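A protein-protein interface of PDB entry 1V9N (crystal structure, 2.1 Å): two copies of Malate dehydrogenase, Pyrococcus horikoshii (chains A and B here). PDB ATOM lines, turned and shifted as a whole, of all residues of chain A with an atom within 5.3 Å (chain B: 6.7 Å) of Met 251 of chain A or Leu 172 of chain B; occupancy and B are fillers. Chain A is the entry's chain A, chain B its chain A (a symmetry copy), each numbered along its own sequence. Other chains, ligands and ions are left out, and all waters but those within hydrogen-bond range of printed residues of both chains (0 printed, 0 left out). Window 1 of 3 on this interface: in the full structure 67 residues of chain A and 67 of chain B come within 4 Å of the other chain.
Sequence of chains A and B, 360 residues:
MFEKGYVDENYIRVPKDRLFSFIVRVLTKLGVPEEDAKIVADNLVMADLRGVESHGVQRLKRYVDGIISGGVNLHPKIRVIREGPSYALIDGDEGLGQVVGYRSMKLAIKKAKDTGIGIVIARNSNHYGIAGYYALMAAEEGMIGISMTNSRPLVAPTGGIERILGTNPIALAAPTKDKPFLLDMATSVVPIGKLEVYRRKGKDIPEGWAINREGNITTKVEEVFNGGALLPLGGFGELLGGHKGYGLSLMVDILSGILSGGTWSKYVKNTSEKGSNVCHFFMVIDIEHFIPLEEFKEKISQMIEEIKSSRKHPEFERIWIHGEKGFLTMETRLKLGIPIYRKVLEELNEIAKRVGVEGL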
ATOM      1  N   MET A 148      -9.573   5.905   2.622  1.00  0.00           N
ATOM      2  CA  MET A 148      -9.640   4.452   2.546  1.00  0.00           C
ATOM      3  C   MET A 148      -9.046   4.051   1.208  1.00  0.00           C
ATOM      4  O   MET A 148      -8.940   4.875   0.289  1.00  0.00           O
ATOM      5  CB  MET A 148     -11.089   3.959   2.564  1.00  0.00           C
ATOM      6  CG  MET A 148     -11.923   4.355   3.761  1.00  0.00           C
ATOM      7  SD  MET A 148     -13.792   3.873   3.434  1.00  0.00           S
ATOM      8  CE  MET A 148     -14.611   5.044   4.750  1.00  0.00           C
ATOM      9  N   ILE A 170      -8.812   1.994   6.934  1.00  0.00           N
ATOM     10  CA  ILE A 170      -9.699   3.123   7.152  1.00  0.00           C
ATOM     11  C   ILE A 170      -8.939   4.102   8.031  1.00  0.00           C
ATOM     12  O   ILE A 170      -8.364   3.709   9.046  1.00  0.00           O
ATOM     13  CB  ILE A 170     -10.980   2.725   7.904  1.00  0.00           C
ATOM     14  CG1 ILE A 170     -11.818   1.775   7.051  1.00  0.00           C
ATOM     15  CG2 ILE A 170     -11.764   3.982   8.276  1.00  0.00           C
ATOM     16  CD1 ILE A 170     -13.049   1.234   7.764  1.00  0.00           C
ATOM     17  N   GLY A 247     -17.136  -7.104   7.118  1.00  0.00           N
ATOM     18  CA  GLY A 247     -18.043  -6.118   6.563  1.00  0.00           C
ATOM     19  C   GLY A 247     -17.336  -4.798   6.304  1.00  0.00           C
ATOM     20  O   GLY A 247     -17.560  -4.158   5.280  1.00  0.00           O
ATOM     21  N   LEU A 248     -16.485  -4.393   7.240  1.00  0.00           N
ATOM     22  CA  LEU A 248     -15.730  -3.151   7.115  1.00  0.00           C
ATOM     23  C   LEU A 248     -14.859  -3.197   5.862  1.00  0.00           C
ATOM     24  O   LEU A 248     -14.679  -2.189   5.177  1.00  0.00           O
ATOM     25  CB  LEU A 248     -14.855  -2.944   8.356  1.00  0.00           C
ATOM     26  CG  LEU A 248     -15.598  -2.640   9.664  1.00  0.00           C
ATOM     27  CD1 LEU A 248     -14.649  -2.775  10.846  1.00  0.00           C
ATOM     28  CD2 LEU A 248     -16.184  -1.231   9.606  1.00  0.00           C
ATOM     29  N   SER A 249     -14.313  -4.372   5.569  1.00  0.00           N
ATOM     30  CA  SER A 249     -13.476  -4.533   4.387  1.00  0.00           C
ATOM     31  C   SER A 249     -14.301  -4.299   3.129  1.00  0.00           C
ATOM     32  O   SER A 249     -13.819  -3.706   2.166  1.00  0.00           O
ATOM     33  CB  SER A 249     -12.861  -5.934   4.345  1.00  0.00           C
ATOM     34  OG  SER A 249     -12.090  -6.096   3.171  1.00  0.00           O
ATOM     35  N   LEU A 250     -15.544  -4.769   3.142  1.00  0.00           N
ATOM     36  CA  LEU A 250     -16.440  -4.599   1.999  1.00  0.00           C
ATOM     37  C   LEU A 250     -16.875  -3.143   1.846  1.00  0.00           C
ATOM     38  O   LEU A 250     -17.018  -2.638   0.734  1.00  0.00           O
ATOM     39  CB  LEU A 250     -17.673  -5.490   2.151  1.00  0.00           C
ATOM     40  CG  LEU A 250     -17.436  -7.002   2.138  1.00  0.00           C
ATOM     41  CD1 LEU A 250     -18.786  -7.712   2.030  1.00  0.00           C
ATOM     42  CD2 LEU A 250     -16.538  -7.388   0.958  1.00  0.00           C
ATOM     43  N   MET A 251     -17.103  -2.477   2.971  1.00  0.00           N
ATOM     44  CA  MET A 251     -17.492  -1.074   2.946  1.00  0.00           C
ATOM     45  C   MET A 251     -16.432  -0.316   2.156  1.00  0.00           C
ATOM     46  O   MET A 251     -16.749   0.478   1.275  1.00  0.00           O
ATOM     47  CB  MET A 251     -17.567  -0.524   4.375  1.00  0.00           C
ATOM     48  CG  MET A 251     -17.819   0.973   4.453  1.00  0.00           C
ATOM     49  SD  MET A 251     -17.968   1.593   6.290  1.00  0.00           S
ATOM     50  CE  MET A 251     -16.108   1.866   6.653  1.00  0.00           C
ATOM     51  N   VAL A 252     -15.167  -0.579   2.468  1.00  0.00           N
ATOM     52  CA  VAL A 252     -14.062   0.076   1.778  1.00  0.00           C
ATOM     53  C   VAL A 252     -14.093  -0.177   0.266  1.00  0.00           C
ATOM     54  O   VAL A 252     -13.941   0.757  -0.525  1.00  0.00           O
ATOM     55  CB  VAL A 252     -12.700  -0.399   2.327  1.00  0.00           C
ATOM     56  CG1 VAL A 252     -11.567   0.139   1.459  1.00  0.00           C
ATOM     57  CG2 VAL A 252     -12.531   0.054   3.758  1.00  0.00           C
ATOM     58  N   ASP A 253     -14.281  -1.434  -0.132  1.00  0.00           N
ATOM     59  CA  ASP A 253     -14.321  -1.788  -1.552  1.00  0.00           C
ATOM     60  C   ASP A 253     -15.540  -1.202  -2.264  1.00  0.00           C
ATOM     61  O   ASP A 253     -15.478  -0.854  -3.441  1.00  0.00           O
ATOM     62  CB  ASP A 253     -14.320  -3.310  -1.731  1.00  0.00           C
ATOM     63  CG  ASP A 253     -12.975  -3.845  -2.199  1.00  0.00           C
ATOM     64  OD1 ASP A 253     -12.378  -3.258  -3.131  1.00  0.00           O
ATOM     65  OD2 ASP A 253     -12.522  -4.865  -1.650  1.00  0.00           O
ATOM     66  N   ILE A 254     -16.654  -1.105  -1.553  1.00  0.00           N
ATOM     67  CA  ILE A 254     -17.865  -0.555  -2.137  1.00  0.00           C
ATOM     68  C   ILE A 254     -17.683   0.947  -2.376  1.00  0.00           C
ATOM     69  O   ILE A 254     -18.032   1.460  -3.438  1.00  0.00           O
ATOM     70  CB  ILE A 254     -19.081  -0.807  -1.212  1.00  0.00           C
ATOM     71  CG1 ILE A 254     -19.396  -2.305  -1.180  1.00  0.00           C
ATOM     72  CG2 ILE A 254     -20.295  -0.015  -1.694  1.00  0.00           C
ATOM     73  CD1 ILE A 254     -20.464  -2.699  -0.164  1.00  0.00           C
ATOM     74  N   LEU A 255     -17.109   1.641  -1.395  1.00  0.00           N
ATOM     75  CA  LEU A 255     -16.895   3.082  -1.509  1.00  0.00           C
ATOM     76  C   LEU A 255     -15.744   3.438  -2.444  1.00  0.00           C
ATOM     77  O   LEU A 255     -15.754   4.490  -3.085  1.00  0.00           O
ATOM     78  CB  LEU A 255     -16.651   3.690  -0.121  1.00  0.00           C
ATOM     79  CG  LEU A 255     -17.845   3.612   0.843  1.00  0.00           C
ATOM     80  CD1 LEU A 255     -17.440   4.121   2.225  1.00  0.00           C
ATOM     81  CD2 LEU A 255     -19.001   4.431   0.294  1.00  0.00           C
ATOM     82  N   SER A 256     -14.756   2.552  -2.528  1.00  0.00           N
ATOM     83  CA  SER A 256     -13.594   2.775  -3.375  1.00  0.00           C
ATOM     84  C   SER A 256     -13.703   2.142  -4.760  1.00  0.00           C
ATOM     85  O   SER A 256     -13.816   2.837  -5.761  1.00  0.00           O
ATOM     86  CB  SER A 256     -12.334   2.229  -2.690  1.00  0.00           C
ATOM     87  OG  SER A 256     -12.111   2.858  -1.440  1.00  0.00           O
ATOM     88  N   ALA B 131     -29.365   1.102  13.401  1.00  0.00           N
ATOM     89  CA  ALA B 131     -28.763   2.053  12.475  1.00  0.00           C
ATOM     90  C   ALA B 131     -29.066   1.677  11.022  1.00  0.00           C
ATOM     91  O   ALA B 131     -29.226   2.547  10.167  1.00  0.00           O
ATOM     92  CB  ALA B 131     -27.249   2.107  12.699  1.00  0.00           C
ATOM     93  N   GLY B 132     -29.157   0.378  10.751  1.00  0.00           N
ATOM     94  CA  GLY B 132     -29.423  -0.073   9.392  1.00  0.00           C
ATOM     95  C   GLY B 132     -30.736   0.426   8.822  1.00  0.00           C
ATOM     96  O   GLY B 132     -30.903   0.522   7.604  1.00  0.00           O
ATOM     97  N   ALA B 135     -29.893   3.631   6.978  1.00  0.00           N
ATOM     98  CA  ALA B 135     -29.039   3.383   5.819  1.00  0.00           C
ATOM     99  C   ALA B 135     -29.875   2.786   4.693  1.00  0.00           C
ATOM    100  O   ALA B 135     -29.702   3.147   3.528  1.00  0.00           O
ATOM    101  CB  ALA B 135     -27.896   2.435   6.182  1.00  0.00           C
ATOM    102  N   LEU B 136     -30.783   1.875   5.047  1.00  0.00           N
ATOM    103  CA  LEU B 136     -31.644   1.215   4.063  1.00  0.00           C
ATOM    104  C   LEU B 136     -32.539   2.181   3.311  1.00  0.00           C
ATOM    105  O   LEU B 136     -32.863   1.961   2.139  1.00  0.00           O
ATOM    106  CB  LEU B 136     -32.516   0.145   4.730  1.00  0.00           C
ATOM    107  CG  LEU B 136     -31.906  -1.252   4.866  1.00  0.00           C
ATOM    108  CD1 LEU B 136     -32.897  -2.171   5.577  1.00  0.00           C
ATOM    109  CD2 LEU B 136     -31.567  -1.806   3.478  1.00  0.00           C
ATOM    110  N   ILE B 144     -26.223   5.059  -1.864  1.00  0.00           N
ATOM    111  CA  ILE B 144     -25.482   4.450  -0.765  1.00  0.00           C
ATOM    112  C   ILE B 144     -25.844   5.226   0.498  1.00  0.00           C
ATOM    113  O   ILE B 144     -25.812   6.460   0.521  1.00  0.00           O
ATOM    114  CB  ILE B 144     -23.957   4.538  -0.970  1.00  0.00           C
ATOM    115  CG1 ILE B 144     -23.546   3.705  -2.189  1.00  0.00           C
ATOM    116  CG2 ILE B 144     -23.231   4.067   0.314  1.00  0.00           C
ATOM    117  CD1 ILE B 144     -22.076   3.790  -2.531  1.00  0.00           C
ATOM    118  N   GLY B 145     -26.209   4.504   1.544  1.00  0.00           N
ATOM    119  CA  GLY B 145     -26.569   5.164   2.778  1.00  0.00           C
ATOM    120  C   GLY B 145     -25.670   4.722   3.912  1.00  0.00           C
ATOM    121  O   GLY B 145     -25.365   3.531   4.056  1.00  0.00           O
ATOM    122  N   ILE B 146     -25.224   5.695   4.699  1.00  0.00           N
ATOM    123  CA  ILE B 146     -24.382   5.430   5.858  1.00  0.00           C
ATOM    124  C   ILE B 146     -25.008   6.112   7.064  1.00  0.00           C
ATOM    125  O   ILE B 146     -25.412   7.279   6.988  1.00  0.00           O
ATOM    126  CB  ILE B 146     -22.957   5.987   5.685  1.00  0.00           C
ATOM    127  CG1 ILE B 146     -22.217   5.208   4.596  1.00  0.00           C
ATOM    128  CG2 ILE B 146     -22.205   5.906   7.016  1.00  0.00           C
ATOM    129  CD1 ILE B 146     -20.889   5.820   4.208  1.00  0.00           C
ATOM    130  N   SER B 147     -25.113   5.378   8.166  1.00  0.00           N
ATOM    131  CA  SER B 147     -25.666   5.946   9.383  1.00  0.00           C
ATOM    132  C   SER B 147     -24.899   5.468  10.603  1.00  0.00           C
ATOM    133  O   SER B 147     -24.446   4.329  10.658  1.00  0.00           O
ATOM    134  CB  SER B 147     -27.140   5.587   9.540  1.00  0.00           C
ATOM    135  OG  SER B 147     -27.675   6.266  10.663  1.00  0.00           O
ATOM    136  N   MET B 148     -24.753   6.360  11.578  1.00  0.00           N
ATOM    137  CA  MET B 148     -24.052   6.065  12.819  1.00  0.00           C
ATOM    138  C   MET B 148     -24.772   6.815  13.924  1.00  0.00           C
ATOM    139  O   MET B 148     -25.522   7.765  13.661  1.00  0.00           O
ATOM    140  CB  MET B 148     -22.612   6.585  12.783  1.00  0.00           C
ATOM    141  CG  MET B 148     -21.733   6.064  11.670  1.00  0.00           C
ATOM    142  SD  MET B 148     -20.055   7.071  11.646  1.00  0.00           S
ATOM    143  CE  MET B 148     -19.508   6.651   9.829  1.00  0.00           C
ATOM    144  N   ILE B 170     -22.260   1.311  13.238  1.00  0.00           N
ATOM    145  CA  ILE B 170     -21.975   1.840  11.916  1.00  0.00           C
ATOM    146  C   ILE B 170     -22.788   1.009  10.938  1.00  0.00           C
ATOM    147  O   ILE B 170     -22.774  -0.220  11.004  1.00  0.00           O
ATOM    148  CB  ILE B 170     -20.494   1.687  11.530  1.00  0.00           C
ATOM    149  CG1 ILE B 170     -19.620   2.539  12.449  1.00  0.00           C
ATOM    150  CG2 ILE B 170     -20.306   2.071  10.065  1.00  0.00           C
ATOM    151  CD1 ILE B 170     -18.127   2.358  12.217  1.00  0.00           C
ATOM    152  N   ALA B 171     -23.499   1.673  10.034  1.00  0.00           N
ATOM    153  CA  ALA B 171     -24.295   0.957   9.052  1.00  0.00           C
ATOM    154  C   ALA B 171     -24.103   1.528   7.653  1.00  0.00           C
ATOM    155  O   ALA B 171     -24.022   2.745   7.477  1.00  0.00           O
ATOM    156  CB  ALA B 171     -25.771   1.009   9.433  1.00  0.00           C
ATOM    157  N   LEU B 172     -24.012   0.637   6.671  1.00  0.00           N
ATOM    158  CA  LEU B 172     -23.883   1.024   5.277  1.00  0.00           C
ATOM    159  C   LEU B 172     -24.771   0.114   4.450  1.00  0.00           C
ATOM    160  O   LEU B 172     -24.708  -1.115   4.559  1.00  0.00           O
ATOM    161  CB  LEU B 172     -22.434   0.914   4.778  1.00  0.00           C
ATOM    162  CG  LEU B 172     -22.238   1.408   3.329  1.00  0.00           C
ATOM    163  CD1 LEU B 172     -20.809   1.883   3.145  1.00  0.00           C
ATOM    164  CD2 LEU B 172     -22.577   0.303   2.328  1.00  0.00           C
ATOM    165  N   ALA B 173     -25.612   0.727   3.630  1.00  0.00           N
ATOM    166  CA  ALA B 173     -26.507  -0.021   2.768  1.00  0.00           C
ATOM    167  C   ALA B 173     -26.258   0.438   1.341  1.00  0.00           C
ATOM    168  O   ALA B 173     -26.050   1.624   1.090  1.00  0.00           O
ATOM    169  CB  ALA B 173     -27.957   0.241   3.161  1.00  0.00           C
ATOM    170  N   ALA B 174     -26.253  -0.505   0.410  1.00  0.00           N
ATOM    171  CA  ALA B 174     -26.053  -0.177  -0.993  1.00  0.00           C
ATOM    172  C   ALA B 174     -27.007  -1.034  -1.814  1.00  0.00           C
ATOM    173  O   ALA B 174     -27.253  -2.188  -1.476  1.00  0.00           O
ATOM    174  CB  ALA B 174     -24.615  -0.458  -1.399  1.00  0.00           C
ATOM    175  N   PHE B 181     -27.358  -4.529   0.002  1.00  0.00           N
ATOM    176  CA  PHE B 181     -26.254  -4.994   0.815  1.00  0.00           C
ATOM    177  C   PHE B 181     -26.507  -4.195   2.093  1.00  0.00           C
ATOM    178  O   PHE B 181     -26.852  -3.016   2.017  1.00  0.00           O
ATOM    179  CB  PHE B 181     -24.923  -4.563   0.200  1.00  0.00           C
ATOM    180  CG  PHE B 181     -23.767  -4.653   1.142  1.00  0.00           C
ATOM    181  CD1 PHE B 181     -23.059  -5.843   1.284  1.00  0.00           C
ATOM    182  CD2 PHE B 181     -23.399  -3.551   1.913  1.00  0.00           C
ATOM    183  CE1 PHE B 181     -21.993  -5.934   2.185  1.00  0.00           C
ATOM    184  CE2 PHE B 181     -22.344  -3.629   2.815  1.00  0.00           C
ATOM    185  CZ  PHE B 181     -21.636  -4.821   2.953  1.00  0.00           C
ATOM    186  N   LEU B 182     -26.351  -4.811   3.255  1.00  0.00           N
ATOM    187  CA  LEU B 182     -26.594  -4.080   4.491  1.00  0.00           C
ATOM    188  C   LEU B 182     -25.701  -4.482   5.648  1.00  0.00           C
ATOM    189  O   LEU B 182     -25.881  -5.540   6.254  1.00  0.00           O
ATOM    190  CB  LEU B 182     -28.060  -4.223   4.917  1.00  0.00           C
ATOM    191  CG  LEU B 182     -28.444  -3.629   6.285  1.00  0.00           C
ATOM    192  CD1 LEU B 182     -28.195  -2.116   6.304  1.00  0.00           C
ATOM    193  CD2 LEU B 182     -29.917  -3.946   6.581  1.00  0.00           C
ATOM    194  N   LEU B 183     -24.717  -3.638   5.928  1.00  0.00           N
ATOM    195  CA  LEU B 183     -23.825  -3.854   7.052  1.00  0.00           C
ATOM    196  C   LEU B 183     -24.447  -3.004   8.154  1.00  0.00           C
ATOM    197  O   LEU B 183     -24.810  -1.851   7.921  1.00  0.00           O
ATOM    198  CB  LEU B 183     -22.417  -3.341   6.738  1.00  0.00           C
ATOM    199  CG  LEU B 183     -21.419  -3.275   7.905  1.00  0.00           C
ATOM    200  CD1 LEU B 183     -21.199  -4.678   8.474  1.00  0.00           C
ATOM    201  CD2 LEU B 183     -20.099  -2.690   7.420  1.00  0.00           C
ATOM    202  N   ASP B 184     -24.602  -3.583   9.337  1.00  0.00           N
ATOM    203  CA  ASP B 184     -25.165  -2.861  10.473  1.00  0.00           C
ATOM    204  C   ASP B 184     -24.554  -3.527  11.695  1.00  0.00           C
ATOM    205  O   ASP B 184     -24.977  -4.607  12.092  1.00  0.00           O
ATOM    206  CB  ASP B 184     -26.695  -2.972  10.490  1.00  0.00           C
ATOM    207  CG  ASP B 184     -27.323  -2.071  11.534  1.00  0.00           C
ATOM    208  OD1 ASP B 184     -26.556  -1.332  12.194  1.00  0.00           O
ATOM    209  OD2 ASP B 184     -28.562  -2.096  11.697  1.00  0.00           O
ATOM    210  N   MET B 185     -23.565  -2.865  12.290  1.00  0.00           N
ATOM    211  CA  MET B 185     -22.828  -3.429  13.415  1.00  0.00           C
ATOM    212  C   MET B 185     -22.429  -2.458  14.519  1.00  0.00           C
ATOM    213  O   MET B 185     -22.092  -1.302  14.258  1.00  0.00           O
ATOM    214  CB  MET B 185     -21.540  -4.044  12.874  1.00  0.00           C
ATOM    215  CG  MET B 185     -20.784  -3.030  12.006  1.00  0.00           C
ATOM    216  SD  MET B 185     -18.960  -3.413  11.536  1.00  0.00           S
ATOM    217  CE  MET B 185     -18.089  -2.622  13.075  1.00  0.00           C
ATOM    218  N   LEU B 248     -12.833   2.872  16.149  1.00  0.00           N
ATOM    219  CA  LEU B 248     -14.073   2.964  15.385  1.00  0.00           C
ATOM    220  C   LEU B 248     -15.162   3.610  16.238  1.00  0.00           C
ATOM    221  O   LEU B 248     -15.987   4.377  15.740  1.00  0.00           O
ATOM    222  CB  LEU B 248     -14.516   1.567  14.938  1.00  0.00           C
ATOM    223  CG  LEU B 248     -13.635   0.884  13.882  1.00  0.00           C
ATOM    224  CD1 LEU B 248     -14.001  -0.589  13.772  1.00  0.00           C
ATOM    225  CD2 LEU B 248     -13.815   1.582  12.536  1.00  0.00           C
ATOM    226  N   MET B 251     -14.513   7.282  16.202  1.00  0.00           N
ATOM    227  CA  MET B 251     -14.844   7.860  14.907  1.00  0.00           C
ATOM    228  C   MET B 251     -16.318   8.243  14.935  1.00  0.00           C
ATOM    229  O   MET B 251     -16.691   9.348  14.550  1.00  0.00           O
ATOM    230  CB  MET B 251     -14.596   6.834  13.794  1.00  0.00           C
ATOM    231  CG  MET B 251     -15.052   7.286  12.417  1.00  0.00           C
ATOM    232  SD  MET B 251     -14.650   5.968  11.046  1.00  0.00           S
ATOM    233  CE  MET B 251     -16.213   4.877  11.227  1.00  0.00           C
ATOM    234  N   HIS B 322     -23.364  -9.481   4.148  1.00  0.00           N
ATOM    235  CA  HIS B 322     -24.018  -8.677   5.168  1.00  0.00           C
ATOM    236  C   HIS B 322     -25.430  -8.245   4.821  1.00  0.00           C
ATOM    237  O   HIS B 322     -25.686  -7.653   3.771  1.00  0.00           O
ATOM    238  CB  HIS B 322     -23.130  -7.488   5.511  1.00  0.00           C
ATOM    239  CG  HIS B 322     -21.761  -7.903   5.942  1.00  0.00           C
ATOM    240  ND1 HIS B 322     -20.837  -8.421   5.063  1.00  0.00           N
ATOM    241  CD2 HIS B 322     -21.197  -7.984   7.170  1.00  0.00           C
ATOM    242  CE1 HIS B 322     -19.764  -8.807   5.730  1.00  0.00           C
ATOM    243  NE2 HIS B 322     -19.957  -8.552   7.012  1.00  0.00           N
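The backbone NH of Gly 247 of chain A lies close to a ring nitrogen (NE2) of His 322 of chain B (3.2 Å).
The backbone NH (N) of Leu 182 of chain B lies within hydrogen-bond range of the backbone carbonyl oxygen (O) of His 322 of chain B. The backbone carbonyl oxygen of Ala 174 of chain B sits at hydrogen-bond distance from the backbone NH of Phe 181 of chain B. O of Met 185 of chain B is in hydrogen-bond range of N of Ile 170 of chain B (2.8 Å). The backbone carbonyl oxygen (O) of Leu 172 of chain B is in hydrogen-bond range of the backbone NH (N) of Leu 183 of chain B, at 2.9 Å.
Among the printed residues, merely in contact across the chains: Met 251 of chain A with Leu 172 of chain B (3.4 Å), Gly 247 of chain A with Leu 183 of chain B (3.6 Å), Ile 254 of chain A with Phe 181 of chain B (3.6 Å), Leu 250 of chain A with Phe 181 of chain B (3.7 Å), Leu 248 of chain A with Leu 248 of chain B (3.7 Å), Leu 250 of chain A with His 322 of chain B (3.7 Å), Leu 248 of chain A with Met 185 of chain B (3.9 Å) and Leu 248 of chain A with Leu 183 of chain B (3.999 Å).
Met 251 of chain A touches just one residue of chain B: Leu 172 (3.4 Å). Printed residues of chain B within 4 Å of Ile 254 of chain A: Phe 181 (3.6 Å). Printed residues of chain A within 4 Å of His 322 of chain B: Gly 247 and Leu 250. Of the printed residues of chain A, Phe 181 of chain B touches Leu 250 and Ile 254. Of the printed residues of chain B, Leu 250 of chain A touches Phe 181 and His 322. Printed residues of chain B within 4 Å of Leu 248 of chain A: Leu 183 (3.999 Å), Met 185 (3.9 Å) and Leu 248 (3.7 Å). Met 251 of chain B touches none of the printed residues of chain A. The nearest residue of chain A that does not touch Leu 172 of chain B is Leu 255 of chain A (4.1 Å).
Printed residues of chain B that touch a printed residue of chain A: Leu 172, Phe 181, Leu 183, Met 185, Leu 248 and His 322. Hydrophobic or aromatic side chains of chain B that line the printed part of chain A: Leu 172, Phe 181, Leu 183, Met 185, Leu 248 and His 322. Of the 12 printed residues of chain A, 5 touch a printed residue of chain B.
Leu 248 of chain A touches its own counterpart, Leu 248 of chain B. Positions printed for both chains: 148, 170, 248 and 251. Of the 9 pairs that touch across the chains among the printed residues, 1 has its exchanged pair printed and touching as well.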
